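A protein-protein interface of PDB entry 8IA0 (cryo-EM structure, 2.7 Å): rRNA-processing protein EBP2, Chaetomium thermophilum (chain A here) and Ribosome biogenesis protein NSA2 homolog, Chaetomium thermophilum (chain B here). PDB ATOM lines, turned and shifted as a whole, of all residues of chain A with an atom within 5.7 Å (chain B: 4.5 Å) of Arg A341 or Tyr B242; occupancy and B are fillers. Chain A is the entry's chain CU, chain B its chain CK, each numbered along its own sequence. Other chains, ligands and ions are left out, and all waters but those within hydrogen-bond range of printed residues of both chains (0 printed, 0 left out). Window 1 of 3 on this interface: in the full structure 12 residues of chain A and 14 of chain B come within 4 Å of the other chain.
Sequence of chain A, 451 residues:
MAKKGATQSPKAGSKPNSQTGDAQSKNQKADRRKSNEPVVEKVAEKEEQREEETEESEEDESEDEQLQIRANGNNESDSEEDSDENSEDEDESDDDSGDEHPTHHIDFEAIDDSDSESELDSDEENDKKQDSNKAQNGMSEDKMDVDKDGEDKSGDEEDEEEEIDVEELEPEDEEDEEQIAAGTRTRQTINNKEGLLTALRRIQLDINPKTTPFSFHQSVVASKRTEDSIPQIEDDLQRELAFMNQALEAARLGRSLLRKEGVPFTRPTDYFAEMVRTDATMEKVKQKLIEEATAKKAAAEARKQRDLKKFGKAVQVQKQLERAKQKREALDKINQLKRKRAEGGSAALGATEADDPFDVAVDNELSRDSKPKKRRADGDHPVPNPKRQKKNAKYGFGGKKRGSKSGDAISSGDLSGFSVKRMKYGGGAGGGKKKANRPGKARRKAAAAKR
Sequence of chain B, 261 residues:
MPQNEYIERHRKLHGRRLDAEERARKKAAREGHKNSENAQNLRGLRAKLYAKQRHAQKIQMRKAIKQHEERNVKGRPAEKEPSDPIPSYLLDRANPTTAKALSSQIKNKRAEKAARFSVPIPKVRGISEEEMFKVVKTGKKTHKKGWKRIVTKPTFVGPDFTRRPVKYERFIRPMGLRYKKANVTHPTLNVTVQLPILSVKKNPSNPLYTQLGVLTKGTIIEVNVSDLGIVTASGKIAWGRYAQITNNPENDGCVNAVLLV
The side-chain carboxylate (OE2) of Glu A353 lies within hydrogen-bond range of the backbone NH (N) of Tyr B242 (2.6 Å). O of Leu B260 sits at hydrogen-bond distance from NH1 of Arg A341 (2.7 Å).
Leu A337 touches Leu B260 (CD2 to CD2, 3.8 Å). Lys A338 touches Leu B260. NH2 of Arg A341 touches CD2 of Tyr B242, 3.6 Å away. CB of Arg A341 touches C of Val B261, 3.9 Å away. Arg B241 touches Leu A349. Glu A353 touches Arg B241 (OE2 to CA, 3.2 Å). CG2 of Ile B220 touches CZ of Phe A358, at 3.9 Å. Tyr B242 touches Phe A358.
Of the printed residues of chain B, Leu A337 touches Leu B260. Lys A340 touches none of the printed residues of chain B. Printed residues of chain B within 4 Å of Arg A341: Tyr B242 (3.6 Å), Leu B260 (2.7 Å) and Val B261 (3.9 Å). Of the printed residues of chain B, Glu A353 touches Arg B241 and Tyr B242. Of the printed residues of chain B, Phe A358 touches Ile B220 and Tyr B242. Ile B221 touches none of the printed residues of chain A. Printed residues of chain A within 4 Å of Tyr B242: Arg A341, Glu A353 and Phe A358. The nearest printed residue of chain B that does not touch Leu A337 is Tyr B242 (4.6 Å).
The backbone NH of Lys B201 lies within hydrogen-bond range of the backbone carbonyl oxygen of Ile B220, at 3.0 Å. The side-chain hydroxyl of Tyr B242 lies within hydrogen-bond range of the side-chain amino group of Lys B201 (3.5 Å). The backbone carbonyl oxygen (O) of Tyr B242 sits at hydrogen-bond distance from the backbone NH (N) of Leu B260. The guanidinium group (NH2) of Arg A341 lies within salt-bridge range of the side-chain carboxylate (OE1) of Glu A353 (3.5 Å). The side-chain carboxylate of Glu A365 is in salt-bridge range of the guanidinium group of Arg A341.
Hydrophobic or aromatic side chains of chain A within 4 Å of the printed part of chain B: Leu A337, Leu A349 and Phe A358. Hydrophobic or aromatic side chains of chain B within 4 Å of the printed part of chain A: Ile B220, Tyr B242 and Leu B260. Among the printed residues, 10 pairs touch across the chains. Among the printed residues, no Asp or Glu carboxylate lies within 4 Å of a Lys or Arg side-chain nitrogen of the other chain.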
ATOM      1  N   GLN A 336       4.821 -11.518  10.883  1.00  0.00           N
ATOM      2  CA  GLN A 336       5.520 -12.230   9.819  1.00  0.00           C
ATOM      3  C   GLN A 336       6.416 -13.323  10.385  1.00  0.00           C
ATOM      4  O   GLN A 336       6.519 -14.413   9.812  1.00  0.00           O
ATOM      5  CB  GLN A 336       6.340 -11.252   8.979  1.00  0.00           C
ATOM      6  CG  GLN A 336       5.614 -10.726   7.759  1.00  0.00           C
ATOM      7  CD  GLN A 336       6.531  -9.969   6.824  1.00  0.00           C
ATOM      8  OE1 GLN A 336       7.405  -9.224   7.263  1.00  0.00           O
ATOM      9  NE2 GLN A 336       6.339 -10.159   5.524  1.00  0.00           N
ATOM     10  N   LEU A 337       7.084 -13.043  11.506  1.00  0.00           N
ATOM     11  CA  LEU A 337       7.900 -14.058  12.157  1.00  0.00           C
ATOM     12  C   LEU A 337       7.044 -15.220  12.642  1.00  0.00           C
ATOM     13  O   LEU A 337       7.475 -16.378  12.606  1.00  0.00           O
ATOM     14  CB  LEU A 337       8.671 -13.440  13.320  1.00  0.00           C
ATOM     15  CG  LEU A 337       9.813 -14.269  13.899  1.00  0.00           C
ATOM     16  CD1 LEU A 337      11.042 -14.141  13.024  1.00  0.00           C
ATOM     17  CD2 LEU A 337      10.122 -13.838  15.321  1.00  0.00           C
ATOM     18  N   LYS A 338       5.827 -14.928  13.107  1.00  0.00           N
ATOM     19  CA  LYS A 338       4.935 -15.981  13.577  1.00  0.00           C
ATOM     20  C   LYS A 338       4.587 -16.955  12.460  1.00  0.00           C
ATOM     21  O   LYS A 338       4.568 -18.172  12.671  1.00  0.00           O
ATOM     22  CB  LYS A 338       3.667 -15.362  14.164  1.00  0.00           C
ATOM     23  CG  LYS A 338       3.702 -15.186  15.670  1.00  0.00           C
ATOM     24  CD  LYS A 338       2.306 -15.013  16.252  1.00  0.00           C
ATOM     25  CE  LYS A 338       1.264 -15.787  15.466  1.00  0.00           C
ATOM     26  NZ  LYS A 338      -0.003 -15.935  16.232  1.00  0.00           N
ATOM     27  N   ARG A 339       4.299 -16.436  11.263  1.00  0.00           N
ATOM     28  CA  ARG A 339       3.995 -17.311  10.135  1.00  0.00           C
ATOM     29  C   ARG A 339       5.204 -18.147   9.741  1.00  0.00           C
ATOM     30  O   ARG A 339       5.073 -19.341   9.447  1.00  0.00           O
ATOM     31  CB  ARG A 339       3.512 -16.488   8.941  1.00  0.00           C
ATOM     32  CG  ARG A 339       2.004 -16.444   8.772  1.00  0.00           C
ATOM     33  CD  ARG A 339       1.400 -15.292   9.546  1.00  0.00           C
ATOM     34  NE  ARG A 339       1.962 -14.012   9.134  1.00  0.00           N
ATOM     35  CZ  ARG A 339       1.533 -13.302   8.100  1.00  0.00           C
ATOM     36  NH1 ARG A 339       0.531 -13.718   7.344  1.00  0.00           N
ATOM     37  NH2 ARG A 339       2.125 -12.144   7.817  1.00  0.00           N
ATOM     38  N   LYS A 340       6.389 -17.534   9.719  1.00  0.00           N
ATOM     39  CA  LYS A 340       7.585 -18.246   9.282  1.00  0.00           C
ATOM     40  C   LYS A 340       7.929 -19.388  10.231  1.00  0.00           C
ATOM     41  O   LYS A 340       8.276 -20.488   9.787  1.00  0.00           O
ATOM     42  CB  LYS A 340       8.757 -17.273   9.161  1.00  0.00           C
ATOM     43  CG  LYS A 340      10.121 -17.937   9.129  1.00  0.00           C
ATOM     44  CD  LYS A 340      10.678 -17.991   7.715  1.00  0.00           C
ATOM     45  CE  LYS A 340      10.519 -16.657   7.003  1.00  0.00           C
ATOM     46  NZ  LYS A 340      10.997 -16.717   5.595  1.00  0.00           N
ATOM     47  N   ARG A 341       7.840 -19.146  11.541  1.00  0.00           N
ATOM     48  CA  ARG A 341       8.110 -20.209  12.501  1.00  0.00           C
ATOM     49  C   ARG A 341       7.080 -21.326  12.387  1.00  0.00           C
ATOM     50  O   ARG A 341       7.428 -22.511  12.460  1.00  0.00           O
ATOM     51  CB  ARG A 341       8.134 -19.646  13.922  1.00  0.00           C
ATOM     52  CG  ARG A 341       9.193 -18.585  14.160  1.00  0.00           C
ATOM     53  CD  ARG A 341      10.448 -19.169  14.778  1.00  0.00           C
ATOM     54  NE  ARG A 341      11.366 -18.128  15.222  1.00  0.00           N
ATOM     55  CZ  ARG A 341      11.641 -17.859  16.490  1.00  0.00           C
ATOM     56  NH1 ARG A 341      11.089 -18.545  17.477  1.00  0.00           N
ATOM     57  NH2 ARG A 341      12.493 -16.880  16.778  1.00  0.00           N
ATOM     58  N   ALA A 342       5.806 -20.969  12.214  1.00  0.00           N
ATOM     59  CA  ALA A 342       4.765 -21.981  12.083  1.00  0.00           C
ATOM     60  C   ALA A 342       4.945 -22.805  10.815  1.00  0.00           C
ATOM     61  O   ALA A 342       4.759 -24.027  10.831  1.00  0.00           O
ATOM     62  CB  ALA A 342       3.386 -21.325  12.104  1.00  0.00           C
ATOM     63  N   GLU A 343       5.301 -22.154   9.706  1.00  0.00           N
ATOM     64  CA  GLU A 343       5.510 -22.878   8.456  1.00  0.00           C
ATOM     65  C   GLU A 343       6.719 -23.800   8.551  1.00  0.00           C
ATOM     66  O   GLU A 343       6.647 -24.976   8.176  1.00  0.00           O
ATOM     67  CB  GLU A 343       5.670 -21.889   7.300  1.00  0.00           C
ATOM     68  CG  GLU A 343       4.372 -21.380   6.639  1.00  0.00           C
ATOM     69  CD  GLU A 343       3.190 -22.351   6.669  1.00  0.00           C
ATOM     70  OE1 GLU A 343       3.382 -23.584   6.566  1.00  0.00           O
ATOM     71  OE2 GLU A 343       2.046 -21.867   6.796  1.00  0.00           O
ATOM     72  N   GLY A 344       7.839 -23.284   9.047  1.00  0.00           N
ATOM     73  CA  GLY A 344       9.028 -24.090   9.235  1.00  0.00           C
ATOM     74  C   GLY A 344      10.163 -23.322   9.880  1.00  0.00           C
ATOM     75  O   GLY A 344      10.498 -22.216   9.446  1.00  0.00           O
ATOM     76  N   GLY A 345      10.768 -23.899  10.913  1.00  0.00           N
ATOM     77  CA  GLY A 345      11.856 -23.247  11.618  1.00  0.00           C
ATOM     78  C   GLY A 345      11.500 -22.837  13.034  1.00  0.00           C
ATOM     79  O   GLY A 345      11.796 -23.553  13.989  1.00  0.00           O
ATOM     80  N   LEU A 349      16.394 -23.387  14.980  1.00  0.00           N
ATOM     81  CA  LEU A 349      16.936 -22.465  15.964  1.00  0.00           C
ATOM     82  C   LEU A 349      17.901 -23.193  16.896  1.00  0.00           C
ATOM     83  O   LEU A 349      18.077 -24.411  16.831  1.00  0.00           O
ATOM     84  CB  LEU A 349      15.808 -21.805  16.759  1.00  0.00           C
ATOM     85  CG  LEU A 349      15.151 -20.567  16.151  1.00  0.00           C
ATOM     86  CD1 LEU A 349      14.114 -20.959  15.111  1.00  0.00           C
ATOM     87  CD2 LEU A 349      14.527 -19.711  17.239  1.00  0.00           C
ATOM     88  N   GLU A 353      17.659 -17.819  22.349  1.00  0.00           N
ATOM     89  CA  GLU A 353      17.422 -16.891  21.256  1.00  0.00           C
ATOM     90  C   GLU A 353      18.658 -16.036  20.998  1.00  0.00           C
ATOM     91  O   GLU A 353      19.586 -15.969  21.811  1.00  0.00           O
ATOM     92  CB  GLU A 353      16.213 -16.005  21.554  1.00  0.00           C
ATOM     93  CG  GLU A 353      14.925 -16.785  21.735  1.00  0.00           C
ATOM     94  CD  GLU A 353      14.180 -16.993  20.432  1.00  0.00           C
ATOM     95  OE1 GLU A 353      14.827 -16.985  19.364  1.00  0.00           O
ATOM     96  OE2 GLU A 353      12.946 -17.178  20.473  1.00  0.00           O
ATOM     97  N   ALA A 354      18.664 -15.384  19.838  1.00  0.00           N
ATOM     98  CA  ALA A 354      19.831 -14.629  19.406  1.00  0.00           C
ATOM     99  C   ALA A 354      20.115 -13.472  20.355  1.00  0.00           C
ATOM    100  O   ALA A 354      19.197 -12.827  20.870  1.00  0.00           O
ATOM    101  CB  ALA A 354      19.621 -14.116  17.982  1.00  0.00           C
ATOM    102  N   ASP A 356      21.611 -10.602  19.747  1.00  0.00           N
ATOM    103  CA  ASP A 356      21.504  -9.269  19.182  1.00  0.00           C
ATOM    104  C   ASP A 356      20.107  -8.697  19.431  1.00  0.00           C
ATOM    105  O   ASP A 356      19.165  -9.442  19.712  1.00  0.00           O
ATOM    106  CB  ASP A 356      21.818  -9.308  17.687  1.00  0.00           C
ATOM    107  CG  ASP A 356      20.989 -10.327  16.944  1.00  0.00           C
ATOM    108  OD1 ASP A 356      20.294 -11.118  17.611  1.00  0.00           O
ATOM    109  OD2 ASP A 356      21.031 -10.341  15.696  1.00  0.00           O
ATOM    110  N   PHE A 358      16.310  -7.087  19.139  1.00  0.00           N
ATOM    111  CA  PHE A 358      15.151  -7.631  18.431  1.00  0.00           C
ATOM    112  C   PHE A 358      14.724  -6.728  17.277  1.00  0.00           C
ATOM    113  O   PHE A 358      13.552  -6.404  17.101  1.00  0.00           O
ATOM    114  CB  PHE A 358      14.006  -7.839  19.416  1.00  0.00           C
ATOM    115  CG  PHE A 358      12.909  -8.732  18.906  1.00  0.00           C
ATOM    116  CD1 PHE A 358      13.080 -10.103  18.856  1.00  0.00           C
ATOM    117  CD2 PHE A 358      11.697  -8.202  18.497  1.00  0.00           C
ATOM    118  CE1 PHE A 358      12.070 -10.924  18.394  1.00  0.00           C
ATOM    119  CE2 PHE A 358      10.688  -9.017  18.034  1.00  0.00           C
ATOM    120  CZ  PHE A 358      10.874 -10.380  17.984  1.00  0.00           C
ATOM    121  N   ALA A 361      17.908  -9.318  14.748  1.00  0.00           N
ATOM    122  CA  ALA A 361      17.623 -10.746  14.842  1.00  0.00           C
ATOM    123  C   ALA A 361      16.431 -11.125  13.973  1.00  0.00           C
ATOM    124  O   ALA A 361      16.452 -12.147  13.280  1.00  0.00           O
ATOM    125  CB  ALA A 361      17.374 -11.135  16.299  1.00  0.00           C
ATOM    126  N   GLU A 365      16.607 -13.367  10.511  1.00  0.00           N
ATOM    127  CA  GLU A 365      15.858 -14.615  10.408  1.00  0.00           C
ATOM    128  C   GLU A 365      14.902 -14.593   9.222  1.00  0.00           C
ATOM    129  O   GLU A 365      14.769 -15.594   8.508  1.00  0.00           O
ATOM    130  CB  GLU A 365      15.107 -14.883  11.712  1.00  0.00           C
ATOM    131  CG  GLU A 365      13.960 -15.869  11.580  1.00  0.00           C
ATOM    132  CD  GLU A 365      13.845 -16.788  12.779  1.00  0.00           C
ATOM    133  OE1 GLU A 365      13.148 -16.425  13.748  1.00  0.00           O
ATOM    134  OE2 GLU A 365      14.454 -17.878  12.752  1.00  0.00           O
ATOM    135  N   LYS B 201      11.917  -8.081  25.297  1.00  0.00           N
ATOM    136  CA  LYS B 201      12.691  -7.829  24.089  1.00  0.00           C
ATOM    137  C   LYS B 201      12.210  -6.610  23.311  1.00  0.00           C
ATOM    138  O   LYS B 201      13.030  -5.794  22.884  1.00  0.00           O
ATOM    139  CB  LYS B 201      12.673  -9.070  23.189  1.00  0.00           C
ATOM    140  CG  LYS B 201      13.254 -10.311  23.847  1.00  0.00           C
ATOM    141  CD  LYS B 201      14.518  -9.984  24.628  1.00  0.00           C
ATOM    142  CE  LYS B 201      15.621 -10.985  24.346  1.00  0.00           C
ATOM    143  NZ  LYS B 201      16.036 -10.958  22.917  1.00  0.00           N
ATOM    144  N   ILE B 220       6.795  -8.598  22.977  1.00  0.00           N
ATOM    145  CA  ILE B 220       7.602  -9.803  22.830  1.00  0.00           C
ATOM    146  C   ILE B 220       8.471  -9.967  24.068  1.00  0.00           C
ATOM    147  O   ILE B 220       9.241  -9.070  24.424  1.00  0.00           O
ATOM    148  CB  ILE B 220       8.458  -9.745  21.560  1.00  0.00           C
ATOM    149  CG1 ILE B 220       7.571  -9.779  20.317  1.00  0.00           C
ATOM    150  CG2 ILE B 220       9.453 -10.890  21.541  1.00  0.00           C
ATOM    151  CD1 ILE B 220       6.861 -11.092  20.116  1.00  0.00           C
ATOM    152  N   ILE B 221       8.348 -11.116  24.728  1.00  0.00           N
ATOM    153  CA  ILE B 221       9.159 -11.447  25.886  1.00  0.00           C
ATOM    154  C   ILE B 221       9.864 -12.771  25.612  1.00  0.00           C
ATOM    155  O   ILE B 221       9.448 -13.562  24.765  1.00  0.00           O
ATOM    156  CB  ILE B 221       8.332 -11.524  27.185  1.00  0.00           C
ATOM    157  CG1 ILE B 221       7.195 -12.533  27.039  1.00  0.00           C
ATOM    158  CG2 ILE B 221       7.784 -10.158  27.549  1.00  0.00           C
ATOM    159  CD1 ILE B 221       6.448 -12.795  28.321  1.00  0.00           C
ATOM    160  N   ARG B 241      12.815 -19.060  24.387  1.00  0.00           N
ATOM    161  CA  ARG B 241      12.121 -18.749  23.148  1.00  0.00           C
ATOM    162  C   ARG B 241      11.288 -17.489  23.330  1.00  0.00           C
ATOM    163  O   ARG B 241      10.921 -17.118  24.447  1.00  0.00           O
ATOM    164  CB  ARG B 241      11.231 -19.911  22.695  1.00  0.00           C
ATOM    165  CG  ARG B 241      11.994 -21.145  22.259  1.00  0.00           C
ATOM    166  CD  ARG B 241      12.527 -20.987  20.852  1.00  0.00           C
ATOM    167  NE  ARG B 241      12.979 -22.254  20.291  1.00  0.00           N
ATOM    168  CZ  ARG B 241      14.208 -22.734  20.413  1.00  0.00           C
ATOM    169  NH1 ARG B 241      15.144 -22.076  21.077  1.00  0.00           N
ATOM    170  NH2 ARG B 241      14.506 -23.903  19.855  1.00  0.00           N
ATOM    171  N   TYR B 242      10.992 -16.836  22.211  1.00  0.00           N
ATOM    172  CA  TYR B 242      10.161 -15.641  22.236  1.00  0.00           C
ATOM    173  C   TYR B 242       8.708 -16.004  22.512  1.00  0.00           C
ATOM    174  O   TYR B 242       8.242 -17.090  22.160  1.00  0.00           O
ATOM    175  CB  TYR B 242      10.261 -14.891  20.908  1.00  0.00           C
ATOM    176  CG  TYR B 242      11.608 -14.261  20.643  1.00  0.00           C
ATOM    177  CD1 TYR B 242      12.248 -13.505  21.614  1.00  0.00           C
ATOM    178  CD2 TYR B 242      12.236 -14.415  19.416  1.00  0.00           C
ATOM    179  CE1 TYR B 242      13.478 -12.929  21.372  1.00  0.00           C
ATOM    180  CE2 TYR B 242      13.466 -13.848  19.167  1.00  0.00           C
ATOM    181  CZ  TYR B 242      14.082 -13.103  20.146  1.00  0.00           C
ATOM    182  OH  TYR B 242      15.308 -12.530  19.900  1.00  0.00           O
ATOM    183  N   ALA B 243       7.989 -15.084  23.149  1.00  0.00           N
ATOM    184  CA  ALA B 243       6.565 -15.236  23.402  1.00  0.00           C
ATOM    185  C   ALA B 243       5.911 -13.864  23.362  1.00  0.00           C
ATOM    186  O   ALA B 243       6.449 -12.899  23.908  1.00  0.00           O
ATOM    187  CB  ALA B 243       6.299 -15.907  24.754  1.00  0.00           C
ATOM    188  N   LEU B 259       3.600 -18.935  22.610  1.00  0.00           N
ATOM    189  CA  LEU B 259       4.981 -19.171  22.216  1.00  0.00           C
ATOM    190  C   LEU B 259       5.146 -19.028  20.708  1.00  0.00           C
ATOM    191  O   LEU B 259       4.319 -19.508  19.926  1.00  0.00           O
ATOM    192  CB  LEU B 259       5.423 -20.560  22.670  1.00  0.00           C
ATOM    193  CG  LEU B 259       6.902 -20.752  22.996  1.00  0.00           C
ATOM    194  CD1 LEU B 259       7.302 -19.878  24.162  1.00  0.00           C
ATOM    195  CD2 LEU B 259       7.186 -22.212  23.305  1.00  0.00           C
ATOM    196  N   LEU B 260       6.223 -18.356  20.302  1.00  0.00           N
ATOM    197  CA  LEU B 260       6.532 -18.150  18.886  1.00  0.00           C
ATOM    198  C   LEU B 260       7.374 -19.327  18.400  1.00  0.00           C
ATOM    199  O   LEU B 260       8.601 -19.262  18.295  1.00  0.00           O
ATOM    200  CB  LEU B 260       7.246 -16.822  18.679  1.00  0.00           C
ATOM    201  CG  LEU B 260       6.416 -15.662  18.130  1.00  0.00           C
ATOM    202  CD1 LEU B 260       5.379 -15.216  19.143  1.00  0.00           C
ATOM    203  CD2 LEU B 260       7.317 -14.504  17.744  1.00  0.00           C
ATOM    204  N   VAL B 261       6.691 -20.427  18.106  1.00  0.00           N
ATOM    205  CA  VAL B 261       7.356 -21.645  17.671  1.00  0.00           C
ATOM    206  C   VAL B 261       6.678 -22.201  16.424  1.00  0.00           C
ATOM    207  O   VAL B 261       5.466 -22.069  16.254  1.00  0.00           O
ATOM    208  CB  VAL B 261       7.378 -22.695  18.794  1.00  0.00           C
ATOM    209  CG1 VAL B 261       7.650 -24.077  18.221  1.00  0.00           C
ATOM    210  CG2 VAL B 261       8.419 -22.331  19.836  1.00  0.00           C
